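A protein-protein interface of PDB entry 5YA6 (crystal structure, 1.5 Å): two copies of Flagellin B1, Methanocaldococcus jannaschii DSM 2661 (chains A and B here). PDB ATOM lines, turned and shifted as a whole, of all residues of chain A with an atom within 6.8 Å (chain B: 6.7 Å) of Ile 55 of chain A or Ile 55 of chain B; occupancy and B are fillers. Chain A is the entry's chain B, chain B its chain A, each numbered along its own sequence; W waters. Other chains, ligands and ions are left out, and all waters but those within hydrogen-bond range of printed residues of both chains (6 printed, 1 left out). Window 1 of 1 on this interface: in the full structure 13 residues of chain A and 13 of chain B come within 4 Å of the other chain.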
ATOM      1  N   PHE A  53      -0.401  29.791   3.672  1.00  0.00           N
ATOM      2  CA  PHE A  53       0.111  29.662   2.287  1.00  0.00           C
ATOM      3  C   PHE A  53      -0.796  30.417   1.375  1.00  0.00           C
ATOM      4  O   PHE A  53      -1.997  30.218   1.459  1.00  0.00           O
ATOM      5  CB  PHE A  53       0.156  28.150   1.914  1.00  0.00           C
ATOM      6  CG  PHE A  53       1.077  27.308   2.782  1.00  0.00           C
ATOM      7  CD1 PHE A  53       2.422  27.102   2.446  1.00  0.00           C
ATOM      8  CD2 PHE A  53       0.609  26.690   3.887  1.00  0.00           C
ATOM      9  CE1 PHE A  53       3.264  26.363   3.282  1.00  0.00           C
ATOM     10  CE2 PHE A  53       1.436  25.924   4.714  1.00  0.00           C
ATOM     11  CZ  PHE A  53       2.771  25.744   4.396  1.00  0.00           C
ATOM     12  N   LEU A  54      -0.281  31.325   0.580  1.00  0.00           N
ATOM     13  CA  LEU A  54      -1.075  32.070  -0.365  1.00  0.00           C
ATOM     14  C   LEU A  54      -0.423  32.103  -1.749  1.00  0.00           C
ATOM     15  O   LEU A  54       0.656  32.656  -1.886  1.00  0.00           O
ATOM     16  CB  LEU A  54      -1.192  33.500   0.082  1.00  0.00           C
ATOM     17  CG  LEU A  54      -1.967  33.749   1.387  1.00  0.00           C
ATOM     18  CD1 LEU A  54      -1.823  35.217   1.810  1.00  0.00           C
ATOM     19  CD2 LEU A  54      -3.429  33.417   1.203  1.00  0.00           C
ATOM     20  N   ILE A  55      -1.141  31.687  -2.781  1.00  0.00           N
ATOM     21  CA  ILE A  55      -0.671  31.809  -4.149  1.00  0.00           C
ATOM     22  C   ILE A  55      -1.382  32.972  -4.849  1.00  0.00           C
ATOM     23  O   ILE A  55      -2.609  33.113  -4.827  1.00  0.00           O
ATOM     24  CB  ILE A  55      -1.018  30.511  -4.939  1.00  0.00           C
ATOM     25  CG1 ILE A  55      -0.443  29.262  -4.304  1.00  0.00           C
ATOM     26  CG2 ILE A  55      -0.579  30.631  -6.426  1.00  0.00           C
ATOM     27  CD1 ILE A  55      -1.171  27.960  -4.623  1.00  0.00           C
ATOM     28  N   TYR A  56      -0.580  33.838  -5.522  1.00  0.00           N
ATOM     29  CA  TYR A  56      -1.128  34.979  -6.244  1.00  0.00           C
ATOM     30  C   TYR A  56      -0.051  35.375  -7.277  1.00  0.00           C
ATOM     31  O   TYR A  56       1.121  35.469  -6.948  1.00  0.00           O
ATOM     32  CB  TYR A  56      -1.568  36.164  -5.290  1.00  0.00           C
ATOM     33  CG  TYR A  56      -1.803  37.430  -6.075  1.00  0.00           C
ATOM     34  CD1 TYR A  56      -2.819  37.542  -6.999  1.00  0.00           C
ATOM     35  CD2 TYR A  56      -0.908  38.519  -5.969  1.00  0.00           C
ATOM     36  CE1 TYR A  56      -2.965  38.641  -7.825  1.00  0.00           C
ATOM     37  CE2 TYR A  56      -1.102  39.654  -6.720  1.00  0.00           C
ATOM     38  CZ  TYR A  56      -2.103  39.736  -7.656  1.00  0.00           C
ATOM     39  OH  TYR A  56      -2.203  40.798  -8.496  1.00  0.00           O
ATOM     40  N   ASP A  57      -0.462  35.548  -8.521  1.00  0.00           N
ATOM     41  CA  ASP A  57       0.345  36.182  -9.536  1.00  0.00           C
ATOM     42  C   ASP A  57       1.655  35.440  -9.739  1.00  0.00           C
ATOM     43  O   ASP A  57       2.676  36.039  -9.861  1.00  0.00           O
ATOM     44  CB  ASP A  57       0.593  37.673  -9.170  1.00  0.00           C
ATOM     45  CG  ASP A  57       1.150  38.509 -10.359  1.00  0.00           C
ATOM     46  OD1 ASP A  57       0.846  38.216 -11.516  1.00  0.00           O
ATOM     47  OD2 ASP A  57       1.916  39.422 -10.097  1.00  0.00           O
ATOM     48  N   GLY A  58       1.594  34.118  -9.760  1.00  0.00           N
ATOM     49  CA  GLY A  58       2.731  33.332 -10.157  1.00  0.00           C
ATOM     50  C   GLY A  58       3.780  33.192  -9.068  1.00  0.00           C
ATOM     51  O   GLY A  58       4.920  32.769  -9.344  1.00  0.00           O
ATOM     52  N   GLU A  59       3.418  33.454  -7.808  1.00  0.00           N
ATOM     53  CA  GLU A  59       4.262  33.208  -6.657  1.00  0.00           C
ATOM     54  C   GLU A  59       3.491  32.571  -5.516  1.00  0.00           C
ATOM     55  O   GLU A  59       2.347  32.897  -5.288  1.00  0.00           O
ATOM     56  CB  GLU A  59       4.918  34.495  -6.090  1.00  0.00           C
ATOM     57  CG  GLU A  59       5.809  35.283  -7.018  1.00  0.00           C
ATOM     58  CD  GLU A  59       6.466  36.481  -6.303  1.00  0.00           C
ATOM     59  OE1 GLU A  59       6.945  36.348  -5.105  1.00  0.00           O
ATOM     60  OE2 GLU A  59       6.443  37.557  -6.932  1.00  0.00           O
ATOM     61  N   SER A  60       4.172  31.755  -4.742  1.00  0.00           N
ATOM     62  CA  SER A  60       3.624  31.139  -3.577  1.00  0.00           C
ATOM     63  C   SER A  60       4.323  31.843  -2.386  1.00  0.00           C
ATOM     64  O   SER A  60       5.506  32.304  -2.498  1.00  0.00           O
ATOM     65  CB  SER A  60       3.930  29.634  -3.582  1.00  0.00           C
ATOM     66  OG  SER A  60       3.239  28.970  -2.531  1.00  0.00           O
ATOM     67  N   HIS A  61       3.536  32.177  -1.373  1.00  0.00           N
ATOM     68  CA  HIS A  61       4.050  32.857  -0.173  1.00  0.00           C
ATOM     69  C   HIS A  61       3.703  32.062   1.019  1.00  0.00           C
ATOM     70  O   HIS A  61       2.578  31.523   1.081  1.00  0.00           O
ATOM     71  CB  HIS A  61       3.441  34.238  -0.047  1.00  0.00           C
ATOM     72  CG  HIS A  61       3.725  35.104  -1.203  1.00  0.00           C
ATOM     73  ND1 HIS A  61       4.805  35.948  -1.242  1.00  0.00           N
ATOM     74  CD2 HIS A  61       3.096  35.237  -2.387  1.00  0.00           C
ATOM     75  CE1 HIS A  61       4.808  36.584  -2.398  1.00  0.00           C
ATOM     76  NE2 HIS A  61       3.785  36.158  -3.113  1.00  0.00           N
ATOM     77  N   PHE A 128       2.682  40.897  -1.455  1.00  0.00           N
ATOM     78  CA  PHE A 128       2.669  40.758  -2.897  1.00  0.00           C
ATOM     79  C   PHE A 128       3.404  41.871  -3.600  1.00  0.00           C
ATOM     80  O   PHE A 128       3.498  41.830  -4.812  1.00  0.00           O
ATOM     81  CB  PHE A 128       1.195  40.683  -3.394  1.00  0.00           C
ATOM     82  CG  PHE A 128       0.365  39.563  -2.757  1.00  0.00           C
ATOM     83  CD1 PHE A 128       0.867  38.293  -2.568  1.00  0.00           C
ATOM     84  CD2 PHE A 128      -0.925  39.808  -2.325  1.00  0.00           C
ATOM     85  CE1 PHE A 128       0.088  37.276  -2.007  1.00  0.00           C
ATOM     86  CE2 PHE A 128      -1.691  38.802  -1.774  1.00  0.00           C
ATOM     87  CZ  PHE A 128      -1.177  37.531  -1.594  1.00  0.00           C
ATOM     88  N   GLU A 137      -7.134  36.143  -9.004  1.00  0.00           N
ATOM     89  CA  GLU A 137      -7.328  34.852  -8.315  1.00  0.00           C
ATOM     90  C   GLU A 137      -6.356  34.731  -7.147  1.00  0.00           C
ATOM     91  O   GLU A 137      -5.136  34.857  -7.300  1.00  0.00           O
ATOM     92  CB  GLU A 137      -7.019  33.676  -9.240  1.00  0.00           C
ATOM     93  CG  GLU A 137      -7.866  33.629 -10.465  1.00  0.00           C
ATOM     94  CD  GLU A 137      -9.272  33.217 -10.220  1.00  0.00           C
ATOM     95  OE1 GLU A 137      -9.739  33.128  -9.055  1.00  0.00           O
ATOM     96  OE2 GLU A 137      -9.973  33.002 -11.243  1.00  0.00           O
ATOM     97  N   VAL A 138      -6.900  34.422  -5.970  1.00  0.00           N
ATOM     98  CA  VAL A 138      -6.116  34.136  -4.786  1.00  0.00           C
ATOM     99  C   VAL A 138      -6.497  32.798  -4.190  1.00  0.00           C
ATOM    100  O   VAL A 138      -7.687  32.540  -4.012  1.00  0.00           O
ATOM    101  CB  VAL A 138      -6.324  35.242  -3.675  1.00  0.00           C
ATOM    102  CG1 VAL A 138      -5.376  34.957  -2.512  1.00  0.00           C
ATOM    103  CG2 VAL A 138      -5.921  36.600  -4.259  1.00  0.00           C
ATOM    104  N   SER A 139      -5.499  31.960  -3.914  1.00  0.00           N
ATOM    105  CA  SER A 139      -5.709  30.576  -3.416  1.00  0.00           C
ATOM    106  C   SER A 139      -4.796  30.361  -2.220  1.00  0.00           C
ATOM    107  O   SER A 139      -3.688  30.917  -2.135  1.00  0.00           O
ATOM    108  CB  SER A 139      -5.367  29.548  -4.511  1.00  0.00           C
ATOM    109  OG  SER A 139      -6.120  29.820  -5.643  1.00  0.00           O
ATOM    110  N   GLY A 140      -5.236  29.611  -1.233  1.00  0.00           N
ATOM    111  CA  GLY A 140      -4.362  29.382  -0.065  1.00  0.00           C
ATOM    112  C   GLY A 140      -4.921  28.405   0.939  1.00  0.00           C
ATOM    113  O   GLY A 140      -6.062  27.968   0.823  1.00  0.00           O
ATOM    114  N   GLN A 141      -4.117  28.075   1.966  1.00  0.00           N
ATOM    115  CA  GLN A 141      -4.543  27.225   3.042  1.00  0.00           C
ATOM    116  C   GLN A 141      -3.860  27.783   4.305  1.00  0.00           C
ATOM    117  O   GLN A 141      -2.751  28.313   4.252  1.00  0.00           O
ATOM    118  CB  GLN A 141      -4.126  25.753   2.865  1.00  0.00           C
ATOM    119  CG  GLN A 141      -4.827  25.121   1.616  1.00  0.00           C
ATOM    120  CD  GLN A 141      -4.564  23.619   1.537  1.00  0.00           C
ATOM    121  OE1 GLN A 141      -3.963  23.033   2.430  1.00  0.00           O
ATOM    122  NE2 GLN A 141      -5.088  22.972   0.474  1.00  0.00           N
ATOM    123  N   GLN A 143      -2.681  26.257   7.771  1.00  0.00           N
ATOM    124  CA  GLN A 143      -2.353  24.935   8.230  1.00  0.00           C
ATOM    125  C   GLN A 143      -1.618  24.998   9.605  1.00  0.00           C
ATOM    126  O   GLN A 143      -0.448  25.300   9.674  1.00  0.00           O
ATOM    127  CB  GLN A 143      -1.427  24.302   7.209  1.00  0.00           C
ATOM    128  CG  GLN A 143      -1.060  22.850   7.576  1.00  0.00           C
ATOM    129  CD  GLN A 143      -2.220  21.912   7.648  1.00  0.00           C
ATOM    130  OE1 GLN A 143      -2.813  21.520   6.617  1.00  0.00           O
ATOM    131  NE2 GLN A 143      -2.598  21.545   8.896  1.00  0.00           N
ATOM    132  N   PHE B  53       1.287  25.479  -9.229  1.00  0.00           N
ATOM    133  CA  PHE B  53       1.475  25.631  -7.794  1.00  0.00           C
ATOM    134  C   PHE B  53       0.419  24.800  -7.069  1.00  0.00           C
ATOM    135  O   PHE B  53      -0.748  24.940  -7.390  1.00  0.00           O
ATOM    136  CB  PHE B  53       1.298  27.094  -7.405  1.00  0.00           C
ATOM    137  CG  PHE B  53       2.349  27.989  -7.944  1.00  0.00           C
ATOM    138  CD1 PHE B  53       3.550  28.153  -7.259  1.00  0.00           C
ATOM    139  CD2 PHE B  53       2.147  28.634  -9.122  1.00  0.00           C
ATOM    140  CE1 PHE B  53       4.534  28.987  -7.783  1.00  0.00           C
ATOM    141  CE2 PHE B  53       3.153  29.469  -9.683  1.00  0.00           C
ATOM    142  CZ  PHE B  53       4.333  29.621  -8.981  1.00  0.00           C
ATOM    143  N   LEU B  54       0.844  23.932  -6.152  1.00  0.00           N
ATOM    144  CA  LEU B  54      -0.025  23.057  -5.402  1.00  0.00           C
ATOM    145  C   LEU B  54       0.331  23.096  -3.926  1.00  0.00           C
ATOM    146  O   LEU B  54       1.496  22.977  -3.557  1.00  0.00           O
ATOM    147  CB  LEU B  54       0.088  21.622  -5.894  1.00  0.00           C
ATOM    148  CG  LEU B  54      -0.418  21.340  -7.305  1.00  0.00           C
ATOM    149  CD1 LEU B  54      -0.040  19.904  -7.712  1.00  0.00           C
ATOM    150  CD2 LEU B  54      -1.876  21.575  -7.510  1.00  0.00           C
ATOM    151  N   ILE B  55      -0.686  23.283  -3.107  1.00  0.00           N
ATOM    152  CA  ILE B  55      -0.552  23.239  -1.668  1.00  0.00           C
ATOM    153  C   ILE B  55      -1.321  22.033  -1.116  1.00  0.00           C
ATOM    154  O   ILE B  55      -2.520  21.834  -1.450  1.00  0.00           O
ATOM    155  CB  ILE B  55      -1.161  24.465  -1.018  1.00  0.00           C
ATOM    156  CG1 ILE B  55      -0.526  25.780  -1.454  1.00  0.00           C
ATOM    157  CG2 ILE B  55      -1.069  24.350   0.526  1.00  0.00           C
ATOM    158  CD1 ILE B  55      -1.392  27.024  -1.219  1.00  0.00           C
ATOM    159  N   TYR B  56      -0.635  21.236  -0.289  1.00  0.00           N
ATOM    160  CA  TYR B  56      -1.238  20.079   0.357  1.00  0.00           C
ATOM    161  C   TYR B  56      -0.425  19.806   1.674  1.00  0.00           C
ATOM    162  O   TYR B  56       0.817  19.756   1.662  1.00  0.00           O
ATOM    163  CB  TYR B  56      -1.192  18.792  -0.544  1.00  0.00           C
ATOM    164  CG  TYR B  56      -1.509  17.544   0.219  1.00  0.00           C
ATOM    165  CD1 TYR B  56      -2.714  17.387   0.886  1.00  0.00           C
ATOM    166  CD2 TYR B  56      -0.515  16.591   0.441  1.00  0.00           C
ATOM    167  CE1 TYR B  56      -2.950  16.292   1.683  1.00  0.00           C
ATOM    168  CE2 TYR B  56      -0.747  15.503   1.226  1.00  0.00           C
ATOM    169  CZ  TYR B  56      -1.949  15.361   1.856  1.00  0.00           C
ATOM    170  OH  TYR B  56      -2.167  14.322   2.702  1.00  0.00           O
ATOM    171  N   ASP B  57      -1.122  19.643   2.786  1.00  0.00           N
ATOM    172  CA  ASP B  57      -0.514  19.135   4.056  1.00  0.00           C
ATOM    173  C   ASP B  57       0.701  19.962   4.486  1.00  0.00           C
ATOM    174  O   ASP B  57       1.773  19.409   4.876  1.00  0.00           O
ATOM    175  CB  ASP B  57      -0.156  17.671   3.969  1.00  0.00           C
ATOM    176  CG  ASP B  57       0.005  17.038   5.358  1.00  0.00           C
ATOM    177  OD1 ASP B  57      -0.553  17.545   6.366  1.00  0.00           O
ATOM    178  OD2 ASP B  57       0.710  16.066   5.409  1.00  0.00           O
ATOM    179  N   GLY B  58       0.576  21.280   4.389  1.00  0.00           N
ATOM    180  CA  GLY B  58       1.607  22.123   5.013  1.00  0.00           C
ATOM    181  C   GLY B  58       2.840  22.337   4.156  1.00  0.00           C
ATOM    182  O   GLY B  58       3.873  22.845   4.660  1.00  0.00           O
ATOM    183  N   GLU B  59       2.726  22.022   2.853  1.00  0.00           N
ATOM    184  CA  GLU B  59       3.785  22.282   1.901  1.00  0.00           C
ATOM    185  C   GLU B  59       3.240  22.849   0.596  1.00  0.00           C
ATOM    186  O   GLU B  59       2.149  22.447   0.136  1.00  0.00           O
ATOM    187  CB  GLU B  59       4.615  21.043   1.628  1.00  0.00           C
ATOM    188  CG  GLU B  59       5.420  20.560   2.825  1.00  0.00           C
ATOM    189  CD  GLU B  59       6.362  19.425   2.476  1.00  0.00           C
ATOM    190  OE1 GLU B  59       6.796  19.322   1.298  1.00  0.00           O
ATOM    191  OE2 GLU B  59       6.697  18.662   3.400  1.00  0.00           O
ATOM    192  N   SER B  60       3.992  23.776   0.040  1.00  0.00           N
ATOM    193  CA  SER B  60       3.676  24.375  -1.272  1.00  0.00           C
ATOM    194  C   SER B  60       4.681  23.832  -2.261  1.00  0.00           C
ATOM    195  O   SER B  60       5.905  23.825  -1.962  1.00  0.00           O
ATOM    196  CB  SER B  60       3.823  25.901  -1.220  1.00  0.00           C
ATOM    197  OG  SER B  60       2.924  26.461  -2.143  1.00  0.00           O
ATOM    198  N   HIS B  61       4.202  23.366  -3.413  1.00  0.00           N
ATOM    199  CA  HIS B  61       5.060  22.760  -4.424  1.00  0.00           C
ATOM    200  C   HIS B  61       4.888  23.484  -5.715  1.00  0.00           C
ATOM    201  O   HIS B  61       3.779  23.949  -6.022  1.00  0.00           O
ATOM    202  CB  HIS B  61       4.641  21.301  -4.627  1.00  0.00           C
ATOM    203  CG  HIS B  61       4.698  20.477  -3.393  1.00  0.00           C
ATOM    204  ND1 HIS B  61       5.835  19.826  -2.979  1.00  0.00           N
ATOM    205  CD2 HIS B  61       3.744  20.189  -2.462  1.00  0.00           C
ATOM    206  CE1 HIS B  61       5.585  19.162  -1.867  1.00  0.00           C
ATOM    207  NE2 HIS B  61       4.319  19.370  -1.528  1.00  0.00           N
ATOM    208  N   PHE B 128       4.064  14.846  -3.534  1.00  0.00           N
ATOM    209  CA  PHE B 128       3.721  14.943  -2.105  1.00  0.00           C
ATOM    210  C   PHE B 128       4.447  13.856  -1.292  1.00  0.00           C
ATOM    211  O   PHE B 128       4.332  13.850  -0.037  1.00  0.00           O
ATOM    212  CB  PHE B 128       2.198  14.784  -1.939  1.00  0.00           C
ATOM    213  CG  PHE B 128       1.373  15.795  -2.695  1.00  0.00           C
ATOM    214  CD1 PHE B 128       1.716  17.138  -2.744  1.00  0.00           C
ATOM    215  CD2 PHE B 128       0.241  15.395  -3.346  1.00  0.00           C
ATOM    216  CE1 PHE B 128       0.952  18.032  -3.467  1.00  0.00           C
ATOM    217  CE2 PHE B 128      -0.567  16.299  -4.013  1.00  0.00           C
ATOM    218  CZ  PHE B 128      -0.199  17.621  -4.089  1.00  0.00           C
ATOM    219  N   GLU B 137      -7.468  18.371   1.534  1.00  0.00           N
ATOM    220  CA  GLU B 137      -7.649  19.629   0.796  1.00  0.00           C
ATOM    221  C   GLU B 137      -6.419  19.857  -0.112  1.00  0.00           C
ATOM    222  O   GLU B 137      -5.296  19.844   0.356  1.00  0.00           O
ATOM    223  CB  GLU B 137      -7.716  20.806   1.754  1.00  0.00           C
ATOM    224  CG  GLU B 137      -8.740  20.703   2.878  1.00  0.00           C
ATOM    225  CD  GLU B 137     -10.148  20.743   2.364  1.00  0.00           C
ATOM    226  OE1 GLU B 137     -11.069  20.625   3.219  1.00  0.00           O
ATOM    227  OE2 GLU B 137     -10.354  20.966   1.153  1.00  0.00           O
ATOM    228  N   VAL B 138      -6.686  20.113  -1.392  1.00  0.00           N
ATOM    229  CA  VAL B 138      -5.630  20.479  -2.342  1.00  0.00           C
ATOM    230  C   VAL B 138      -6.053  21.770  -3.020  1.00  0.00           C
ATOM    231  O   VAL B 138      -7.171  21.890  -3.524  1.00  0.00           O
ATOM    232  CB  VAL B 138      -5.385  19.362  -3.347  1.00  0.00           C
ATOM    233  CG1 VAL B 138      -4.334  19.798  -4.368  1.00  0.00           C
ATOM    234  CG2 VAL B 138      -4.943  18.068  -2.621  1.00  0.00           C
ATOM    235  N   SER B 139      -5.154  22.749  -3.015  1.00  0.00           N
ATOM    236  CA  SER B 139      -5.432  24.073  -3.547  1.00  0.00           C
ATOM    237  C   SER B 139      -4.281  24.389  -4.503  1.00  0.00           C
ATOM    238  O   SER B 139      -3.144  23.981  -4.307  1.00  0.00           O
ATOM    239  CB  SER B 139      -5.429  25.118  -2.420  1.00  0.00           C
ATOM    240  OG  SER B 139      -6.291  24.741  -1.420  1.00  0.00           O
ATOM    241  N   GLY B 140      -4.562  25.089  -5.579  1.00  0.00           N
ATOM    242  CA  GLY B 140      -3.492  25.439  -6.495  1.00  0.00           C
ATOM    243  C   GLY B 140      -3.877  26.362  -7.604  1.00  0.00           C
ATOM    244  O   GLY B 140      -5.044  26.708  -7.767  1.00  0.00           O
ATOM    245  N   GLN B 141      -2.878  26.793  -8.394  1.00  0.00           N
ATOM    246  CA  GLN B 141      -3.119  27.615  -9.550  1.00  0.00           C
ATOM    247  C   GLN B 141      -2.164  27.163 -10.632  1.00  0.00           C
ATOM    248  O   GLN B 141      -1.000  26.835 -10.351  1.00  0.00           O
ATOM    249  CB  GLN B 141      -2.874  29.099  -9.301  1.00  0.00           C
ATOM    250  CG  GLN B 141      -3.882  29.674  -8.292  1.00  0.00           C
ATOM    251  CD  GLN B 141      -3.797  31.181  -8.162  1.00  0.00           C
ATOM    252  OE1 GLN B 141      -3.036  31.854  -8.831  1.00  0.00           O
ATOM    253  NE2 GLN B 141      -4.611  31.744  -7.262  1.00  0.00           N
ATOM    254  N   GLN B 143      -0.417  28.840 -13.726  1.00  0.00           N
ATOM    255  CA  GLN B 143      -0.102  30.220 -14.126  1.00  0.00           C
ATOM    256  C   GLN B 143       0.897  30.267 -15.293  1.00  0.00           C
ATOM    257  O   GLN B 143       2.078  30.082 -15.137  1.00  0.00           O
ATOM    258  CB  GLN B 143       0.484  30.966 -12.898  1.00  0.00           C
ATOM    259  CG  GLN B 143       0.814  32.424 -13.236  1.00  0.00           C
ATOM    260  CD  GLN B 143      -0.404  33.241 -13.513  1.00  0.00           C
ATOM    261  OE1 GLN B 143      -1.243  33.508 -12.623  1.00  0.00           O
ATOM    262  NE2 GLN B 143      -0.634  33.524 -14.787  1.00  0.00           N
HETATM  263  O   HOH W   1      -3.958  20.239   2.667  1.00  0.00           O
HETATM  264  O   HOH W   2      -0.097  19.716   7.978  1.00  0.00           O
HETATM  265  O   HOH W   3      -2.998  18.750   6.702  1.00  0.00           O
HETATM  266  O   HOH W   4      -3.184  34.654  -9.089  1.00  0.00           O
HETATM  267  O   HOH W   5      -0.598  32.435 -10.143  1.00  0.00           O
HETATM  268  O   HOH W   6      -1.852  22.684   4.228  1.00  0.00           O
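Printed residues of chain B that touch a printed residue of chain A: Phe 53, Ile 55, Gly 58, Ser 60, Glu 137, Val 138, Ser 139, Gly 140, Gln 141 and Gln 143.
The side-chain hydroxyl (OG) of Ser 139 of chain B lies within hydrogen-bond range of the side-chain amide nitrogen (NE2) of Gln 141 of chain A, 2.9 Å away. NE2 of Gln 141 of chain B lies within hydrogen-bond range of OG of Ser 139 of chain A, at 2.9 Å. The side-chain amide nitrogen (NE2) of Gln 141 of chain A sits at hydrogen-bond distance from the backbone carbonyl oxygen (O) of Glu 137 of chain B. The backbone carbonyl oxygen (O) of Ile 55 of chain B is in hydrogen-bond range of the side-chain amide nitrogen (NE2) of Gln 141 of chain A. The side-chain hydroxyl (OG) of Ser 60 of chain B lies within hydrogen-bond range of the side-chain hydroxyl (OG) of Ser 60 of chain A, at 2.6 Å. NE2 of Gln 141 of chain B lies within hydrogen-bond range of O of Glu 137 of chain A (3.2 Å). O of Ile 55 of chain A is in hydrogen-bond range of NE2 of Gln 141 of chain B (3.4 Å).
Water W4 lies within hydrogen-bond range of the backbone carbonyl oxygen (O) of Glu 137 of chain A, the side-chain amide oxygen (OE1) of Gln 141 of chain B and the backbone NH (N) of Asp 57 of chain A. Water W1 lies within hydrogen-bond range of O of Glu 137 of chain B (2.7 Å), OE1 of Gln 141 of chain A (2.8 Å) and N of Asp 57 of chain B (2.9 Å). Water W2 lies within hydrogen-bond range of OD1 of Asp 57 of chain B and NE2 of Gln 143 of chain A. Water W3 lies within hydrogen-bond range of OD1 of Asp 57 of chain B and OE1 of Gln 143 of chain A. Water W5 lies within hydrogen-bond range of the side-chain amide oxygen of Gln 143 of chain B (2.8 Å), the backbone NH of Gly 58 of chain A (2.8 Å) and the side-chain amide oxygen of Gln 141 of chain B (2.8 Å). Water W6 lies within hydrogen-bond range of OE1 of Gln 141 of chain A (2.8 Å), N of Gly 58 of chain B (2.8 Å), OE1 of Gln 143 of chain A (2.8 Å) and N of Asp 57 of chain B (3.4 Å).
The backbone NH (N) of Ile 55 of chain A sits at hydrogen-bond distance from the backbone carbonyl oxygen (O) of Ser 139 of chain A. The backbone NH (N) of Phe 53 of chain A sits at hydrogen-bond distance from the backbone carbonyl oxygen (O) of Gln 141 of chain A (2.8 Å). N of Ile 55 of chain B sits at hydrogen-bond distance from O of Ser 139 of chain B (2.8 Å). The backbone carbonyl oxygen of Gln 141 of chain B lies within hydrogen-bond range of the backbone NH of Phe 53 of chain B (2.9 Å).
Ser 60 of chain A touches Phe 53 of chain B, but with the chains exchanged Phe 53 of chain A does not touch Ser 60 of chain B (4.1 Å). Ser 60 of chain A touches its own counterpart, Ser 60 of chain B. Val 138 of chain A touches Gln 141 of chain B, and with the chains exchanged Gln 141 of chain A touches Val 138 of chain B. Ser 139 of chain A touches Gln 141 of chain B, and with the chains exchanged Gln 141 of chain A touches Ser 139 of chain B.
Among the printed residues, pairs that only touch across the chains: Phe 53 of chain A with Gly 58 of chain B, Gly 58 of chain A with Phe 53 of chain B, Ile 55 of chain A with Ile 55 of chain B, Phe 53 of chain A with Ile 55 of chain B, Gly 58 of chain A with Gln 143 of chain B, Val 138 of chain A with Gln 141 of chain B, Gln 141 of chain A with Val 138 of chain B, Gln 143 of chain A with Gly 58 of chain B, Ile 55 of chain A with Phe 53 of chain B, Ile 55 of chain A with Gly 140 of chain B, Ser 139 of chain A with Gly 140 of chain B, Gly 140 of chain A with Ser 139 of chain B, Gly 140 of chain A with Ile 55 of chain B and Ser 60 of chain A with Phe 53 of chain B.
Of chain A, only Phe 53, Ile 55, Gly 140 and Gln 141 come within 4 Å of Ile 55 of chain B. Printed residues of chain B within 4 Å of Val 138 of chain A: Gln 141 (3.8 Å). Of the printed residues of chain A, Gln 143 of chain B touches Gly 58 (3.7 Å). Of the printed residues of chain A, Ser 139 of chain B touches Gly 140 (3.9 Å) and Gln 141 (2.9 Å). Printed residues of chain B within 4 Å of Gly 58 of chain A: Phe 53 and Gln 143. Phe 128 of chain B touches none of the printed residues of chain A. Phe 128 of chain A touches none of the printed residues of chain B. The nearest residue of chain A that does not touch Ile 55 of chain B is Ser 139 of chain A (4.6 Å). The nearest printed residue of chain A that does not touch Gln 141 of chain B is Tyr 56 of chain A (4.5 Å).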
